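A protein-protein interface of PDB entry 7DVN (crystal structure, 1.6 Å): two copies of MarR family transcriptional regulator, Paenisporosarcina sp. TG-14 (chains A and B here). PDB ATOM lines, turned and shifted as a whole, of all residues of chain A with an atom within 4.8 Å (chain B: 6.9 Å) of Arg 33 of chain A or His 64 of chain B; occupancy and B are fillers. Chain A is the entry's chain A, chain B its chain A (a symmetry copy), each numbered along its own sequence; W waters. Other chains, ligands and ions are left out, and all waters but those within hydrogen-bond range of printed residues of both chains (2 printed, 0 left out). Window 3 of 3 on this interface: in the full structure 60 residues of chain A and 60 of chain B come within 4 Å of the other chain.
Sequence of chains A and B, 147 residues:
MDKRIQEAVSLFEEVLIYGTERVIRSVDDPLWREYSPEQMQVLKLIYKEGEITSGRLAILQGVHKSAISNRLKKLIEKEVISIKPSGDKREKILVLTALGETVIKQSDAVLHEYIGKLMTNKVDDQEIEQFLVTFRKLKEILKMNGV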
ATOM      1  N   ASP A  28     -13.628  16.865 -16.166  1.00  0.00           N
ATOM      2  CA  ASP A  28     -14.647  17.553 -15.328  1.00  0.00           C
ATOM      3  C   ASP A  28     -16.048  17.642 -15.986  1.00  0.00           C
ATOM      4  O   ASP A  28     -17.063  17.884 -15.269  1.00  0.00           O
ATOM      5  CB  ASP A  28     -14.121  18.951 -14.992  1.00  0.00           C
ATOM      6  CG  ASP A  28     -14.916  19.628 -13.898  1.00  0.00           C
ATOM      7  OD1 ASP A  28     -15.774  18.954 -13.305  1.00  0.00           O
ATOM      8  OD2 ASP A  28     -14.642  20.812 -13.624  1.00  0.00           O
ATOM      9  N   ASP A  29     -16.161  17.390 -17.283  1.00  0.00           N
ATOM     10  CA  ASP A  29     -17.318  17.809 -18.097  1.00  0.00           C
ATOM     11  C   ASP A  29     -18.569  17.060 -17.674  1.00  0.00           C
ATOM     12  O   ASP A  29     -18.553  15.828 -17.436  1.00  0.00           O
ATOM     13  CB  ASP A  29     -17.001  17.558 -19.585  1.00  0.00           C
ATOM     14  CG  ASP A  29     -17.954  18.288 -20.510  1.00  0.00           C
ATOM     15  OD1 ASP A  29     -19.099  17.782 -20.711  1.00  0.00           O
ATOM     16  OD2 ASP A  29     -17.567  19.395 -21.030  1.00  0.00           O
ATOM     17  N   PRO A  30     -19.756  17.715 -17.570  1.00  0.00           N
ATOM     18  CA  PRO A  30     -20.968  17.000 -17.220  1.00  0.00           C
ATOM     19  C   PRO A  30     -21.256  15.813 -18.120  1.00  0.00           C
ATOM     20  O   PRO A  30     -21.847  14.869 -17.684  1.00  0.00           O
ATOM     21  CB  PRO A  30     -22.061  18.086 -17.339  1.00  0.00           C
ATOM     22  CG  PRO A  30     -21.331  19.301 -16.987  1.00  0.00           C
ATOM     23  CD  PRO A  30     -19.963  19.172 -17.629  1.00  0.00           C
ATOM     24  N   LEU A  31     -20.880  15.914 -19.402  1.00  0.00           N
ATOM     25  CA  LEU A  31     -21.253  14.826 -20.333  1.00  0.00           C
ATOM     26  C   LEU A  31     -20.482  13.573 -19.923  1.00  0.00           C
ATOM     27  O   LEU A  31     -20.975  12.509 -20.230  1.00  0.00           O
ATOM     28  CB  LEU A  31     -20.965  15.210 -21.780  1.00  0.00           C
ATOM     29  CG  LEU A  31     -21.788  16.371 -22.337  1.00  0.00           C
ATOM     30  CD1 LEU A  31     -21.346  16.688 -23.745  1.00  0.00           C
ATOM     31  CD2 LEU A  31     -23.262  16.088 -22.273  1.00  0.00           C
ATOM     32  N   TRP A  32     -19.280  13.723 -19.360  1.00  0.00           N
ATOM     33  CA  TRP A  32     -18.470  12.526 -18.959  1.00  0.00           C
ATOM     34  C   TRP A  32     -18.914  12.026 -17.583  1.00  0.00           C
ATOM     35  O   TRP A  32     -18.265  11.108 -17.032  1.00  0.00           O
ATOM     36  CB  TRP A  32     -16.969  12.865 -19.011  1.00  0.00           C
ATOM     37  CG  TRP A  32     -16.355  12.589 -20.336  1.00  0.00           C
ATOM     38  CD1 TRP A  32     -16.329  13.392 -21.430  1.00  0.00           C
ATOM     39  CD2 TRP A  32     -15.789  11.349 -20.757  1.00  0.00           C
ATOM     40  NE1 TRP A  32     -15.749  12.769 -22.490  1.00  0.00           N
ATOM     41  CE2 TRP A  32     -15.411  11.495 -22.112  1.00  0.00           C
ATOM     42  CE3 TRP A  32     -15.513  10.173 -20.076  1.00  0.00           C
ATOM     43  CZ2 TRP A  32     -14.772  10.474 -22.810  1.00  0.00           C
ATOM     44  CZ3 TRP A  32     -14.887   9.165 -20.765  1.00  0.00           C
ATOM     45  CH2 TRP A  32     -14.530   9.313 -22.114  1.00  0.00           C
ATOM     46  N   ARG A  33     -19.982  12.593 -17.016  1.00  0.00           N
ATOM     47  CA  ARG A  33     -20.698  12.000 -15.875  1.00  0.00           C
ATOM     48  C   ARG A  33     -22.001  11.405 -16.363  1.00  0.00           C
ATOM     49  O   ARG A  33     -22.333  10.256 -15.992  1.00  0.00           O
ATOM     50  CB  ARG A  33     -20.895  13.036 -14.767  1.00  0.00           C
ATOM     51  CG  ARG A  33     -19.611  13.488 -14.098  1.00  0.00           C
ATOM     52  CD  ARG A  33     -19.874  14.378 -12.900  1.00  0.00           C
ATOM     53  NE  ARG A  33     -20.232  15.736 -13.274  1.00  0.00           N
ATOM     54  CZ  ARG A  33     -19.370  16.670 -13.655  1.00  0.00           C
ATOM     55  NH1 ARG A  33     -19.802  17.893 -13.939  1.00  0.00           N
ATOM     56  NH2 ARG A  33     -18.076  16.395 -13.733  1.00  0.00           N
ATOM     57  N   GLU A  34     -22.733  12.112 -17.224  1.00  0.00           N
ATOM     58  CA  GLU A  34     -24.066  11.680 -17.681  1.00  0.00           C
ATOM     59  C   GLU A  34     -23.934  10.420 -18.519  1.00  0.00           C
ATOM     60  O   GLU A  34     -24.814   9.522 -18.415  1.00  0.00           O
ATOM     61  CB  GLU A  34     -24.773  12.787 -18.470  1.00  0.00           C
ATOM     62  CG  GLU A  34     -26.157  12.328 -18.901  1.00  0.00           C
ATOM     63  CD  GLU A  34     -27.163  13.362 -19.404  1.00  0.00           C
ATOM     64  OE1 GLU A  34     -26.788  14.545 -19.426  1.00  0.00           O
ATOM     65  OE2 GLU A  34     -28.310  12.939 -19.772  1.00  0.00           O
ATOM     66  N   TYR A  35     -22.991  10.446 -19.452  1.00  0.00           N
ATOM     67  CA  TYR A  35     -22.850   9.394 -20.466  1.00  0.00           C
ATOM     68  C   TYR A  35     -21.627   8.559 -20.079  1.00  0.00           C
ATOM     69  O   TYR A  35     -20.532   9.101 -19.897  1.00  0.00           O
ATOM     70  CB  TYR A  35     -22.745   9.977 -21.880  1.00  0.00           C
ATOM     71  CG  TYR A  35     -24.014  10.684 -22.304  1.00  0.00           C
ATOM     72  CD1 TYR A  35     -25.074   9.987 -22.852  1.00  0.00           C
ATOM     73  CD2 TYR A  35     -24.159  12.029 -22.019  1.00  0.00           C
ATOM     74  CE1 TYR A  35     -26.268  10.624 -23.159  1.00  0.00           C
ATOM     75  CE2 TYR A  35     -25.338  12.675 -22.334  1.00  0.00           C
ATOM     76  CZ  TYR A  35     -26.388  11.971 -22.882  1.00  0.00           C
ATOM     77  OH  TYR A  35     -27.556  12.625 -23.203  1.00  0.00           O
ATOM     78  N   SER A  36     -21.812   7.252 -19.982  1.00  0.00           N
ATOM     79  CA  SER A  36     -20.754   6.238 -19.794  1.00  0.00           C
ATOM     80  C   SER A  36     -19.924   6.218 -21.070  1.00  0.00           C
ATOM     81  O   SER A  36     -20.407   6.454 -22.171  1.00  0.00           O
ATOM     82  CB  SER A  36     -21.429   4.919 -19.482  1.00  0.00           C
ATOM     83  OG  SER A  36     -21.992   4.375 -20.646  1.00  0.00           O
ATOM     84  N   GLN A  39     -21.956   4.103 -23.627  1.00  0.00           N
ATOM     85  CA  GLN A  39     -23.040   4.858 -24.288  1.00  0.00           C
ATOM     86  C   GLN A  39     -22.445   5.728 -25.400  1.00  0.00           C
ATOM     87  O   GLN A  39     -22.983   5.753 -26.500  1.00  0.00           O
ATOM     88  CB  GLN A  39     -23.715   5.698 -23.230  1.00  0.00           C
ATOM     89  CG  GLN A  39     -24.596   4.891 -22.321  1.00  0.00           C
ATOM     90  CD  GLN A  39     -25.218   5.645 -21.180  1.00  0.00           C
ATOM     91  OE1 GLN A  39     -24.681   6.624 -20.638  1.00  0.00           O
ATOM     92  NE2 GLN A  39     -26.418   5.195 -20.801  1.00  0.00           N
ATOM     93  N   SER B  54     -17.395  -3.912  -7.379  1.00  0.00           N
ATOM     94  CA  SER B  54     -18.403  -3.539  -8.398  1.00  0.00           C
ATOM     95  C   SER B  54     -18.113  -2.117  -8.948  1.00  0.00           C
ATOM     96  O   SER B  54     -18.273  -1.915 -10.165  1.00  0.00           O
ATOM     97  CB  SER B  54     -19.773  -3.679  -7.843  1.00  0.00           C
ATOM     98  OG  SER B  54     -20.172  -5.014  -7.976  1.00  0.00           O
ATOM     99  N   ALA B  58     -16.832  -1.003 -12.786  1.00  0.00           N
ATOM    100  CA  ALA B  58     -17.668  -0.136 -13.627  1.00  0.00           C
ATOM    101  C   ALA B  58     -16.784   0.882 -14.351  1.00  0.00           C
ATOM    102  O   ALA B  58     -16.898   0.993 -15.599  1.00  0.00           O
ATOM    103  CB  ALA B  58     -18.696   0.560 -12.756  1.00  0.00           C
ATOM    104  N   ILE B  59     -15.944   1.562 -13.577  1.00  0.00           N
ATOM    105  CA  ILE B  59     -14.984   2.571 -14.100  1.00  0.00           C
ATOM    106  C   ILE B  59     -14.031   1.933 -15.135  1.00  0.00           C
ATOM    107  O   ILE B  59     -13.845   2.524 -16.221  1.00  0.00           O
ATOM    108  CB  ILE B  59     -14.245   3.242 -12.950  1.00  0.00           C
ATOM    109  CG1 ILE B  59     -15.267   4.103 -12.203  1.00  0.00           C
ATOM    110  CG2 ILE B  59     -13.097   4.081 -13.467  1.00  0.00           C
ATOM    111  CD1 ILE B  59     -14.827   4.552 -10.863  1.00  0.00           C
ATOM    112  N   GLY B  62     -15.948   1.216 -18.307  1.00  0.00           N
ATOM    113  CA  GLY B  62     -16.637   2.384 -18.878  1.00  0.00           C
ATOM    114  C   GLY B  62     -18.142   2.210 -18.846  1.00  0.00           C
ATOM    115  O   GLY B  62     -18.781   2.523 -19.872  1.00  0.00           O
ATOM    116  N   VAL B  63     -18.658   1.649 -17.746  1.00  0.00           N
ATOM    117  CA  VAL B  63     -20.122   1.362 -17.506  1.00  0.00           C
ATOM    118  C   VAL B  63     -20.599   2.186 -16.315  1.00  0.00           C
ATOM    119  O   VAL B  63     -19.871   2.407 -15.361  1.00  0.00           O
ATOM    120  CB  VAL B  63     -20.294  -0.150 -17.230  1.00  0.00           C
ATOM    121  CG1 VAL B  63     -21.669  -0.508 -16.663  1.00  0.00           C
ATOM    122  CG2 VAL B  63     -19.982  -0.945 -18.498  1.00  0.00           C
ATOM    123  N   HIS B  64     -21.836   2.672 -16.330  1.00  0.00           N
ATOM    124  CA  HIS B  64     -22.418   3.304 -15.131  1.00  0.00           C
ATOM    125  C   HIS B  64     -22.458   2.290 -13.983  1.00  0.00           C
ATOM    126  O   HIS B  64     -22.844   1.136 -14.273  1.00  0.00           O
ATOM    127  CB  HIS B  64     -23.848   3.767 -15.450  1.00  0.00           C
ATOM    128  CG  HIS B  64     -23.914   5.032 -16.250  1.00  0.00           C
ATOM    129  ND1 HIS B  64     -23.355   6.199 -15.801  1.00  0.00           N
ATOM    130  CD2 HIS B  64     -24.496   5.308 -17.439  1.00  0.00           C
ATOM    131  CE1 HIS B  64     -23.617   7.165 -16.688  1.00  0.00           C
ATOM    132  NE2 HIS B  64     -24.302   6.643 -17.686  1.00  0.00           N
ATOM    133  N   LYS B  65     -22.115   2.712 -12.771  1.00  0.00           N
ATOM    134  CA  LYS B  65     -22.205   1.879 -11.542  1.00  0.00           C
ATOM    135  C   LYS B  65     -23.605   1.264 -11.479  1.00  0.00           C
ATOM    136  O   LYS B  65     -23.726   0.064 -11.229  1.00  0.00           O
ATOM    137  CB  LYS B  65     -21.895   2.708 -10.290  1.00  0.00           C
ATOM    138  CG  LYS B  65     -22.180   2.033  -8.955  1.00  0.00           C
ATOM    139  CD  LYS B  65     -21.232   0.929  -8.603  1.00  0.00           C
ATOM    140  CE  LYS B  65     -21.507   0.322  -7.237  1.00  0.00           C
ATOM    141  NZ  LYS B  65     -20.940   1.143  -6.141  1.00  0.00           N
ATOM    142  N   SER B  66     -24.645   2.055 -11.713  1.00  0.00           N
ATOM    143  CA  SER B  66     -26.051   1.551 -11.633  1.00  0.00           C
ATOM    144  C   SER B  66     -26.269   0.304 -12.505  1.00  0.00           C
ATOM    145  O   SER B  66     -27.179  -0.470 -12.164  1.00  0.00           O
ATOM    146  CB  SER B  66     -27.048   2.642 -11.999  1.00  0.00           C
ATOM    147  OG  SER B  66     -26.832   3.136 -13.313  1.00  0.00           O
ATOM    148  N   ALA B  67     -25.528   0.105 -13.611  1.00  0.00           N
ATOM    149  CA  ALA B  67     -25.753  -0.993 -14.593  1.00  0.00           C
ATOM    150  C   ALA B  67     -24.980  -2.260 -14.211  1.00  0.00           C
ATOM    151  O   ALA B  67     -25.300  -3.340 -14.745  1.00  0.00           O
ATOM    152  CB  ALA B  67     -25.361  -0.551 -15.973  1.00  0.00           C
ATOM    153  N   ILE B  68     -24.013  -2.146 -13.316  1.00  0.00           N
ATOM    154  CA  ILE B  68     -23.038  -3.264 -13.197  1.00  0.00           C
ATOM    155  C   ILE B  68     -23.683  -4.449 -12.451  1.00  0.00           C
ATOM    156  O   ILE B  68     -23.427  -5.606 -12.841  1.00  0.00           O
ATOM    157  CB  ILE B  68     -21.709  -2.731 -12.624  1.00  0.00           C
ATOM    158  CG1 ILE B  68     -20.529  -3.579 -13.100  1.00  0.00           C
ATOM    159  CG2 ILE B  68     -21.750  -2.576 -11.115  1.00  0.00           C
ATOM    160  CD1 ILE B  68     -20.155  -3.353 -14.520  1.00  0.00           C
ATOM    161  N   SER B  69     -24.619  -4.238 -11.515  1.00  0.00           N
ATOM    162  CA  SER B  69     -25.279  -5.306 -10.729  1.00  0.00           C
ATOM    163  C   SER B  69     -25.887  -6.354 -11.650  1.00  0.00           C
ATOM    164  O   SER B  69     -25.583  -7.542 -11.474  1.00  0.00           O
ATOM    165  CB  SER B  69     -26.317  -4.740  -9.783  1.00  0.00           C
ATOM    166  OG  SER B  69     -26.932  -5.792  -9.047  1.00  0.00           O
ATOM    167  N   ARG B  71     -25.512  -7.029 -14.744  1.00  0.00           N
ATOM    168  CA  ARG B  71     -24.502  -7.726 -15.591  1.00  0.00           C
ATOM    169  C   ARG B  71     -23.784  -8.808 -14.782  1.00  0.00           C
ATOM    170  O   ARG B  71     -23.584  -9.947 -15.326  1.00  0.00           O
ATOM    171  CB  ARG B  71     -23.529  -6.704 -16.143  1.00  0.00           C
ATOM    172  CG  ARG B  71     -24.269  -5.707 -17.010  1.00  0.00           C
ATOM    173  CD  ARG B  71     -23.382  -4.824 -17.793  1.00  0.00           C
ATOM    174  NE  ARG B  71     -24.189  -3.725 -18.299  1.00  0.00           N
ATOM    175  CZ  ARG B  71     -23.713  -2.763 -19.053  1.00  0.00           C
ATOM    176  NH1 ARG B  71     -22.434  -2.781 -19.393  1.00  0.00           N
ATOM    177  NH2 ARG B  71     -24.523  -1.786 -19.455  1.00  0.00           N
HETATM  178  O   HOH W   1     -23.476   2.218 -19.076  1.00  0.00           O
HETATM  179  O   HOH W   2     -26.879   8.894 -17.249  1.00  0.00           O
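The backbone carbonyl oxygen (O) of Glu 34 of chain A lies within hydrogen-bond range of a ring nitrogen (NE2) of His 64 of chain B (3.0 Å). N of Ser 36 of chain A sits at hydrogen-bond distance from NE2 of His 64 of chain B, at 3.4 Å. A ring nitrogen (NE2) of His 64 of chain B lies within hydrogen-bond range of the side-chain amide oxygen (OE1) of Gln 39 of chain A, 3.0 Å away.
The side-chain carboxylate (OD1) of Asp 28 of chain A lies within salt-bridge range of the guanidinium group (NH2) of Arg 33 of chain A. The backbone NH (N) of Gln 39 of chain A sits at hydrogen-bond distance from the side-chain hydroxyl (OG) of Ser 36 of chain A.
His 64 of chain B touches Arg 33 of chain A (CE1 to O, 3.4 Å). O of Gly 62 of chain B touches CB of Ser 36 of chain A, 3.6 Å away.
Trp 32 of chain A touches none of the printed residues of chain B. Printed residues of chain B within 4 Å of Arg 33 of chain A: His 64. Printed residues of chain B within 4 Å of Glu 34 of chain A: His 64 (3.0 Å). Of the printed residues of chain B, Ser 36 of chain A touches Gly 62 and His 64. Of the printed residues of chain B, Gln 39 of chain A touches His 64 (3.0 Å). Of the printed residues of chain A, Gly 62 of chain B touches Ser 36. The nearest residue of chain A that does not touch His 64 of chain B is Tyr 35 of chain A (4.1 Å). The nearest printed residue of chain A that does not touch Gly 62 of chain B is Gln 39 of chain A (5.2 Å).
Of the 12 printed residues of chain B, 2 touch a printed residue of chain A. Among the printed residues, 5 pairs touch across the chains.
No position is printed for both chains.
Water W2 lies within hydrogen-bond range of O of Glu 34 of chain A (2.5 Å) and NE2 of His 64 of chain B (3.4 Å). Water W1 lies within hydrogen-bond range of OG of Ser 36 of chain A (3.1 Å) and N of His 64 of chain B (3.2 Å).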
